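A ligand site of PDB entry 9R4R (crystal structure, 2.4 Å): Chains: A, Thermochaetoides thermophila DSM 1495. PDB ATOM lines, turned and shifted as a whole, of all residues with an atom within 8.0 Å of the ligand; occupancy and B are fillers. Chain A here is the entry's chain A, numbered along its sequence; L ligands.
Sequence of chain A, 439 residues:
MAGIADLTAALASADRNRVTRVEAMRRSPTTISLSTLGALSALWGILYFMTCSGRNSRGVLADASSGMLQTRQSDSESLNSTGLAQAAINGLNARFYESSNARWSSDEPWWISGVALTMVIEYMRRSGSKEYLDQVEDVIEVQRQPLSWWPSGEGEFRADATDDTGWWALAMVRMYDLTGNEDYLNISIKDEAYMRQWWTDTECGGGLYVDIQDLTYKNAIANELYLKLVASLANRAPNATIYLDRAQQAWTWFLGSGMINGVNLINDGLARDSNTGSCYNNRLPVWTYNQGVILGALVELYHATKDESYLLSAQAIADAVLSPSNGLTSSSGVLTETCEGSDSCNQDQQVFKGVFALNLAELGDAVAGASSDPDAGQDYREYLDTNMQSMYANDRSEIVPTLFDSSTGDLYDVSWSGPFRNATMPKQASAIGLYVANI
OD2 of Asp 164 is in salt-bridge range of N1 of the ligand, at 3.7 Å. O5 of the ligand lies within hydrogen-bond range of OD1 of Asp 348 (3.3 Å). The side-chain carboxylate of Asp 163 sits at hydrogen-bond distance from an oxygen (O2) of the ligand (3.5 Å). The side-chain carboxylate of Asp 160 is in salt-bridge range of a nitrogen (N1) of the ligand (3.6 Å).
N of Asp 348 sits at hydrogen-bond distance from OD1 of Asn 346. The backbone carbonyl oxygen of Ala 161 sits at hydrogen-bond distance from the side-chain hydroxyl of Thr 165.
Merely in contact with the ligand: Pro 109 (3.3 Å), Trp 111 (3.3 Å) and Ala 161 (3.5 Å). Seven residues have an atom within 4 Å of the ligand: Pro 109, Trp 111, Asp 160, Ala 161, Asp 163, Asp 164 and Asp 348.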
ATOM      1  N   GLU A 108      18.545 -10.083 -17.515  1.00  0.00           N
ATOM      2  CA  GLU A 108      17.991 -10.207 -16.179  1.00  0.00           C
ATOM      3  C   GLU A 108      18.106  -8.889 -15.431  1.00  0.00           C
ATOM      4  O   GLU A 108      18.839  -7.985 -15.843  1.00  0.00           O
ATOM      5  CB  GLU A 108      18.732 -11.319 -15.411  1.00  0.00           C
ATOM      6  CG  GLU A 108      18.583 -12.701 -16.043  1.00  0.00           C
ATOM      7  CD  GLU A 108      17.261 -13.382 -15.701  1.00  0.00           C
ATOM      8  OE1 GLU A 108      16.349 -12.708 -15.197  1.00  0.00           O
ATOM      9  OE2 GLU A 108      17.145 -14.594 -15.964  1.00  0.00           O
ATOM     10  N   PRO A 109      17.366  -8.715 -14.326  1.00  0.00           N
ATOM     11  CA  PRO A 109      17.413  -7.435 -13.601  1.00  0.00           C
ATOM     12  C   PRO A 109      18.827  -7.050 -13.186  1.00  0.00           C
ATOM     13  O   PRO A 109      19.618  -7.877 -12.743  1.00  0.00           O
ATOM     14  CB  PRO A 109      16.520  -7.699 -12.377  1.00  0.00           C
ATOM     15  CG  PRO A 109      15.563  -8.722 -12.842  1.00  0.00           C
ATOM     16  CD  PRO A 109      16.298  -9.597 -13.810  1.00  0.00           C
ATOM     17  N   TRP A 110      19.123  -5.752 -13.348  1.00  0.00           N
ATOM     18  CA  TRP A 110      20.453  -5.238 -13.061  1.00  0.00           C
ATOM     19  C   TRP A 110      20.858  -5.470 -11.603  1.00  0.00           C
ATOM     20  O   TRP A 110      22.026  -5.750 -11.319  1.00  0.00           O
ATOM     21  CB  TRP A 110      20.499  -3.750 -13.405  1.00  0.00           C
ATOM     22  CG  TRP A 110      21.791  -3.061 -13.086  1.00  0.00           C
ATOM     23  CD1 TRP A 110      22.972  -3.189 -13.744  1.00  0.00           C
ATOM     24  CD2 TRP A 110      22.018  -2.107 -12.048  1.00  0.00           C
ATOM     25  NE1 TRP A 110      23.925  -2.383 -13.178  1.00  0.00           N
ATOM     26  CE2 TRP A 110      23.364  -1.705 -12.130  1.00  0.00           C
ATOM     27  CE3 TRP A 110      21.214  -1.553 -11.046  1.00  0.00           C
ATOM     28  CZ2 TRP A 110      23.927  -0.780 -11.247  1.00  0.00           C
ATOM     29  CZ3 TRP A 110      21.776  -0.631 -10.173  1.00  0.00           C
ATOM     30  CH2 TRP A 110      23.121  -0.259 -10.278  1.00  0.00           C
ATOM     31  N   TRP A 111      19.898  -5.366 -10.678  1.00  0.00           N
ATOM     32  CA  TRP A 111      20.225  -5.475  -9.263  1.00  0.00           C
ATOM     33  C   TRP A 111      20.651  -6.888  -8.860  1.00  0.00           C
ATOM     34  O   TRP A 111      21.296  -7.054  -7.832  1.00  0.00           O
ATOM     35  CB  TRP A 111      19.038  -5.025  -8.408  1.00  0.00           C
ATOM     36  CG  TRP A 111      17.862  -5.954  -8.449  1.00  0.00           C
ATOM     37  CD1 TRP A 111      16.825  -5.933  -9.341  1.00  0.00           C
ATOM     38  CD2 TRP A 111      17.576  -7.032  -7.543  1.00  0.00           C
ATOM     39  NE1 TRP A 111      15.924  -6.925  -9.059  1.00  0.00           N
ATOM     40  CE2 TRP A 111      16.357  -7.615  -7.964  1.00  0.00           C
ATOM     41  CE3 TRP A 111      18.229  -7.558  -6.429  1.00  0.00           C
ATOM     42  CZ2 TRP A 111      15.794  -8.703  -7.297  1.00  0.00           C
ATOM     43  CZ3 TRP A 111      17.667  -8.634  -5.776  1.00  0.00           C
ATOM     44  CH2 TRP A 111      16.459  -9.199  -6.203  1.00  0.00           C
ATOM     45  N   ILE A 112      20.302  -7.897  -9.657  1.00  0.00           N
ATOM     46  CA  ILE A 112      20.710  -9.261  -9.328  1.00  0.00           C
ATOM     47  C   ILE A 112      22.184  -9.474  -9.650  1.00  0.00           C
ATOM     48  O   ILE A 112      22.852 -10.304  -9.021  1.00  0.00           O
ATOM     49  CB  ILE A 112      19.812 -10.287 -10.042  1.00  0.00           C
ATOM     50  CG1 ILE A 112      18.338  -9.943  -9.807  1.00  0.00           C
ATOM     51  CG2 ILE A 112      20.100 -11.694  -9.558  1.00  0.00           C
ATOM     52  CD1 ILE A 112      17.379 -11.014 -10.259  1.00  0.00           C
ATOM     53  N   TRP A 149      19.608   4.270 -18.027  1.00  0.00           N
ATOM     54  CA  TRP A 149      18.204   4.443 -17.715  1.00  0.00           C
ATOM     55  C   TRP A 149      17.960   5.392 -16.555  1.00  0.00           C
ATOM     56  O   TRP A 149      16.790   5.655 -16.217  1.00  0.00           O
ATOM     57  CB  TRP A 149      17.542   3.088 -17.433  1.00  0.00           C
ATOM     58  CG  TRP A 149      18.061   2.379 -16.219  1.00  0.00           C
ATOM     59  CD1 TRP A 149      17.541   2.436 -14.958  1.00  0.00           C
ATOM     60  CD2 TRP A 149      19.175   1.476 -16.147  1.00  0.00           C
ATOM     61  NE1 TRP A 149      18.271   1.637 -14.105  1.00  0.00           N
ATOM     62  CE2 TRP A 149      19.278   1.042 -14.811  1.00  0.00           C
ATOM     63  CE3 TRP A 149      20.098   1.014 -17.086  1.00  0.00           C
ATOM     64  CZ2 TRP A 149      20.267   0.161 -14.392  1.00  0.00           C
ATOM     65  CZ3 TRP A 149      21.087   0.134 -16.667  1.00  0.00           C
ATOM     66  CH2 TRP A 149      21.157  -0.286 -15.331  1.00  0.00           C
ATOM     67  N   ALA A 159      20.586   4.599  -8.648  1.00  0.00           N
ATOM     68  CA  ALA A 159      19.652   4.188  -9.689  1.00  0.00           C
ATOM     69  C   ALA A 159      18.287   4.834  -9.479  1.00  0.00           C
ATOM     70  O   ALA A 159      18.125   5.775  -8.695  1.00  0.00           O
ATOM     71  CB  ALA A 159      19.551   2.661  -9.714  1.00  0.00           C
ATOM     72  N   ASP A 160      17.293   4.338 -10.216  1.00  0.00           N
ATOM     73  CA  ASP A 160      15.934   4.849 -10.180  1.00  0.00           C
ATOM     74  C   ASP A 160      15.071   4.160  -9.128  1.00  0.00           C
ATOM     75  O   ASP A 160      13.858   4.408  -9.072  1.00  0.00           O
ATOM     76  CB  ASP A 160      15.281   4.718 -11.556  1.00  0.00           C
ATOM     77  CG  ASP A 160      15.127   3.279 -12.004  1.00  0.00           C
ATOM     78  OD1 ASP A 160      15.749   2.378 -11.391  1.00  0.00           O
ATOM     79  OD2 ASP A 160      14.396   3.041 -12.985  1.00  0.00           O
ATOM     80  N   ALA A 161      15.648   3.302  -8.300  1.00  0.00           N
ATOM     81  CA  ALA A 161      14.953   2.665  -7.192  1.00  0.00           C
ATOM     82  C   ALA A 161      15.908   2.563  -6.017  1.00  0.00           C
ATOM     83  O   ALA A 161      17.100   2.304  -6.202  1.00  0.00           O
ATOM     84  CB  ALA A 161      14.422   1.273  -7.578  1.00  0.00           C
ATOM     85  N   THR A 162      15.385   2.792  -4.811  1.00  0.00           N
ATOM     86  CA  THR A 162      16.252   2.814  -3.635  1.00  0.00           C
ATOM     87  C   THR A 162      16.759   1.426  -3.271  1.00  0.00           C
ATOM     88  O   THR A 162      17.822   1.301  -2.659  1.00  0.00           O
ATOM     89  CB  THR A 162      15.516   3.434  -2.441  1.00  0.00           C
ATOM     90  OG1 THR A 162      14.271   2.756  -2.236  1.00  0.00           O
ATOM     91  CG2 THR A 162      15.256   4.913  -2.687  1.00  0.00           C
ATOM     92  N   ASP A 163      16.028   0.366  -3.634  1.00  0.00           N
ATOM     93  CA  ASP A 163      16.504  -0.981  -3.329  1.00  0.00           C
ATOM     94  C   ASP A 163      17.545  -1.437  -4.350  1.00  0.00           C
ATOM     95  O   ASP A 163      18.485  -2.153  -3.989  1.00  0.00           O
ATOM     96  CB  ASP A 163      15.332  -1.962  -3.263  1.00  0.00           C
ATOM     97  CG  ASP A 163      14.496  -1.979  -4.529  1.00  0.00           C
ATOM     98  OD1 ASP A 163      14.703  -1.107  -5.399  1.00  0.00           O
ATOM     99  OD2 ASP A 163      13.635  -2.865  -4.647  1.00  0.00           O
ATOM    100  N   ASP A 164      17.394  -1.048  -5.614  1.00  0.00           N
ATOM    101  CA  ASP A 164      18.436  -1.314  -6.602  1.00  0.00           C
ATOM    102  C   ASP A 164      19.771  -0.745  -6.153  1.00  0.00           C
ATOM    103  O   ASP A 164      20.809  -1.407  -6.228  1.00  0.00           O
ATOM    104  CB  ASP A 164      18.034  -0.746  -7.962  1.00  0.00           C
ATOM    105  CG  ASP A 164      16.953  -1.561  -8.643  1.00  0.00           C
ATOM    106  OD1 ASP A 164      16.144  -2.171  -7.923  1.00  0.00           O
ATOM    107  OD2 ASP A 164      16.903  -1.576  -9.887  1.00  0.00           O
ATOM    108  N   THR A 165      19.762   0.515  -5.685  1.00  0.00           N
ATOM    109  CA  THR A 165      20.972   1.103  -5.129  1.00  0.00           C
ATOM    110  C   THR A 165      21.434   0.360  -3.887  1.00  0.00           C
ATOM    111  O   THR A 165      22.644   0.167  -3.685  1.00  0.00           O
ATOM    112  CB  THR A 165      20.723   2.578  -4.800  1.00  0.00           C
ATOM    113  OG1 THR A 165      20.298   3.272  -5.981  1.00  0.00           O
ATOM    114  CG2 THR A 165      21.983   3.235  -4.258  1.00  0.00           C
ATOM    115  N   TRP A 167      21.338  -2.793  -2.941  1.00  0.00           N
ATOM    116  CA  TRP A 167      22.071  -4.037  -3.130  1.00  0.00           C
ATOM    117  C   TRP A 167      23.525  -3.787  -3.522  1.00  0.00           C
ATOM    118  O   TRP A 167      24.430  -4.452  -3.013  1.00  0.00           O
ATOM    119  CB  TRP A 167      21.382  -4.907  -4.188  1.00  0.00           C
ATOM    120  CG  TRP A 167      20.043  -5.430  -3.781  1.00  0.00           C
ATOM    121  CD1 TRP A 167      18.821  -5.032  -4.235  1.00  0.00           C
ATOM    122  CD2 TRP A 167      19.775  -6.475  -2.824  1.00  0.00           C
ATOM    123  NE1 TRP A 167      17.820  -5.743  -3.628  1.00  0.00           N
ATOM    124  CE2 TRP A 167      18.385  -6.639  -2.757  1.00  0.00           C
ATOM    125  CE3 TRP A 167      20.589  -7.273  -2.015  1.00  0.00           C
ATOM    126  CZ2 TRP A 167      17.777  -7.569  -1.918  1.00  0.00           C
ATOM    127  CZ3 TRP A 167      19.994  -8.208  -1.186  1.00  0.00           C
ATOM    128  CH2 TRP A 167      18.592  -8.348  -1.146  1.00  0.00           C
ATOM    129  N   VAL A 210      10.439   3.008  -2.234  1.00  0.00           N
ATOM    130  CA  VAL A 210      11.214   2.204  -3.164  1.00  0.00           C
ATOM    131  C   VAL A 210      11.127   2.745  -4.583  1.00  0.00           C
ATOM    132  O   VAL A 210      12.112   2.714  -5.323  1.00  0.00           O
ATOM    133  CB  VAL A 210      10.746   0.724  -3.096  1.00  0.00           C
ATOM    134  CG1 VAL A 210       9.244   0.618  -3.311  1.00  0.00           C
ATOM    135  CG2 VAL A 210      11.497  -0.124  -4.115  1.00  0.00           C
ATOM    136  N   ASP A 211       9.965   3.282  -4.958  1.00  0.00           N
ATOM    137  CA  ASP A 211       9.728   3.806  -6.309  1.00  0.00           C
ATOM    138  C   ASP A 211      10.057   5.288  -6.305  1.00  0.00           C
ATOM    139  O   ASP A 211       9.235   6.116  -5.908  1.00  0.00           O
ATOM    140  CB  ASP A 211       8.283   3.544  -6.731  1.00  0.00           C
ATOM    141  CG  ASP A 211       7.310   3.738  -5.587  1.00  0.00           C
ATOM    142  OD1 ASP A 211       7.742   3.670  -4.418  1.00  0.00           O
ATOM    143  OD2 ASP A 211       6.114   3.952  -5.860  1.00  0.00           O
ATOM    144  N   ILE A 212      11.253   5.619  -6.776  1.00  0.00           N
ATOM    145  CA  ILE A 212      11.743   6.995  -6.746  1.00  0.00           C
ATOM    146  C   ILE A 212      10.886   7.886  -7.625  1.00  0.00           C
ATOM    147  O   ILE A 212      10.619   9.046  -7.282  1.00  0.00           O
ATOM    148  CB  ILE A 212      13.230   7.007  -7.161  1.00  0.00           C
ATOM    149  CG1 ILE A 212      14.109   6.712  -5.954  1.00  0.00           C
ATOM    150  CG2 ILE A 212      13.605   8.342  -7.773  1.00  0.00           C
ATOM    151  CD1 ILE A 212      15.589   6.806  -6.224  1.00  0.00           C
ATOM    152  N   ASN A 219       8.040  -0.358   1.191  1.00  0.00           N
ATOM    153  CA  ASN A 219       8.054  -1.798   1.357  1.00  0.00           C
ATOM    154  C   ASN A 219       9.141  -2.220   2.349  1.00  0.00           C
ATOM    155  O   ASN A 219       9.854  -1.391   2.933  1.00  0.00           O
ATOM    156  CB  ASN A 219       8.215  -2.495   0.006  1.00  0.00           C
ATOM    157  CG  ASN A 219       9.585  -2.270  -0.628  1.00  0.00           C
ATOM    158  OD1 ASN A 219      10.437  -1.583  -0.078  1.00  0.00           O
ATOM    159  ND2 ASN A 219       9.785  -2.859  -1.795  1.00  0.00           N
ATOM    160  N   ILE A 221      11.847  -4.579   1.863  1.00  0.00           N
ATOM    161  CA  ILE A 221      13.213  -4.874   1.422  1.00  0.00           C
ATOM    162  C   ILE A 221      14.030  -3.596   1.285  1.00  0.00           C
ATOM    163  O   ILE A 221      15.224  -3.573   1.598  1.00  0.00           O
ATOM    164  CB  ILE A 221      13.191  -5.696   0.130  1.00  0.00           C
ATOM    165  CG1 ILE A 221      14.605  -6.207  -0.197  1.00  0.00           C
ATOM    166  CG2 ILE A 221      12.608  -4.900  -1.035  1.00  0.00           C
ATOM    167  CD1 ILE A 221      15.223  -7.023   0.927  1.00  0.00           C
ATOM    168  N   TYR A 289      13.977 -13.460   1.531  1.00  0.00           N
ATOM    169  CA  TYR A 289      15.025 -12.447   1.641  1.00  0.00           C
ATOM    170  C   TYR A 289      14.590 -11.272   2.527  1.00  0.00           C
ATOM    171  O   TYR A 289      15.445 -10.486   2.935  1.00  0.00           O
ATOM    172  CB  TYR A 289      15.450 -11.969   0.249  1.00  0.00           C
ATOM    173  CG  TYR A 289      14.547 -10.984  -0.471  1.00  0.00           C
ATOM    174  CD1 TYR A 289      13.175 -10.982  -0.285  1.00  0.00           C
ATOM    175  CD2 TYR A 289      15.093 -10.056  -1.354  1.00  0.00           C
ATOM    176  CE1 TYR A 289      12.360 -10.075  -0.956  1.00  0.00           C
ATOM    177  CE2 TYR A 289      14.292  -9.152  -2.026  1.00  0.00           C
ATOM    178  CZ  TYR A 289      12.933  -9.163  -1.827  1.00  0.00           C
ATOM    179  OH  TYR A 289      12.132  -8.259  -2.499  1.00  0.00           O
ATOM    180  N   ASN A 346       9.274 -15.993 -10.201  1.00  0.00           N
ATOM    181  CA  ASN A 346       9.767 -15.160 -11.290  1.00  0.00           C
ATOM    182  C   ASN A 346      11.271 -14.901 -11.116  1.00  0.00           C
ATOM    183  O   ASN A 346      11.923 -15.468 -10.242  1.00  0.00           O
ATOM    184  CB  ASN A 346       8.942 -13.866 -11.373  1.00  0.00           C
ATOM    185  CG  ASN A 346       9.090 -12.980 -10.138  1.00  0.00           C
ATOM    186  OD1 ASN A 346       9.932 -13.213  -9.276  1.00  0.00           O
ATOM    187  ND2 ASN A 346       8.246 -11.965 -10.060  1.00  0.00           N
ATOM    188  N   GLN A 347      11.824 -14.021 -11.955  1.00  0.00           N
ATOM    189  CA  GLN A 347      13.271 -13.792 -11.943  1.00  0.00           C
ATOM    190  C   GLN A 347      13.739 -13.164 -10.632  1.00  0.00           C
ATOM    191  O   GLN A 347      14.889 -13.375 -10.228  1.00  0.00           O
ATOM    192  CB  GLN A 347      13.666 -12.908 -13.126  1.00  0.00           C
ATOM    193  CG  GLN A 347      13.250 -11.450 -13.019  1.00  0.00           C
ATOM    194  CD  GLN A 347      11.810 -11.204 -13.422  1.00  0.00           C
ATOM    195  OE1 GLN A 347      10.923 -11.983 -13.095  1.00  0.00           O
ATOM    196  NE2 GLN A 347      11.587 -10.126 -14.161  1.00  0.00           N
ATOM    197  N   ASP A 348      12.882 -12.398  -9.962  1.00  0.00           N
ATOM    198  CA  ASP A 348      13.260 -11.845  -8.659  1.00  0.00           C
ATOM    199  C   ASP A 348      13.249 -12.926  -7.583  1.00  0.00           C
ATOM    200  O   ASP A 348      14.236 -13.108  -6.860  1.00  0.00           O
ATOM    201  CB  ASP A 348      12.310 -10.703  -8.276  1.00  0.00           C
ATOM    202  CG  ASP A 348      12.354  -9.546  -9.252  1.00  0.00           C
ATOM    203  OD1 ASP A 348      13.395  -9.381  -9.927  1.00  0.00           O
ATOM    204  OD2 ASP A 348      11.362  -8.806  -9.340  1.00  0.00           O
HETATM  205  C1  LIG L   1      13.405  -2.471 -11.704  1.00  0.00           C
HETATM  206  O1  LIG L   1      14.753  -2.316 -11.804  1.00  0.00           O
HETATM  207  C2  LIG L   1      12.908  -1.706 -10.469  1.00  0.00           C
HETATM  208  N1  LIG L   1      13.515  -0.332 -10.497  1.00  0.00           N
HETATM  209  C3  LIG L   1      13.269  -2.366  -9.193  1.00  0.00           C
HETATM  210  O2  LIG L   1      12.568  -1.714  -8.097  1.00  0.00           O
HETATM  211  C4  LIG L   1      12.928  -3.840  -9.176  1.00  0.00           C
HETATM  212  O3  LIG L   1      13.472  -4.427  -7.988  1.00  0.00           O
HETATM  213  C5  LIG L   1      13.493  -4.568 -10.390  1.00  0.00           C
HETATM  214  O4  LIG L   1      13.069  -3.938 -11.658  1.00  0.00           O
HETATM  215  C6  LIG L   1      13.019  -5.988 -10.378  1.00  0.00           C
HETATM  216  O5  LIG L   1      13.312  -6.597 -11.605  1.00  0.00           O
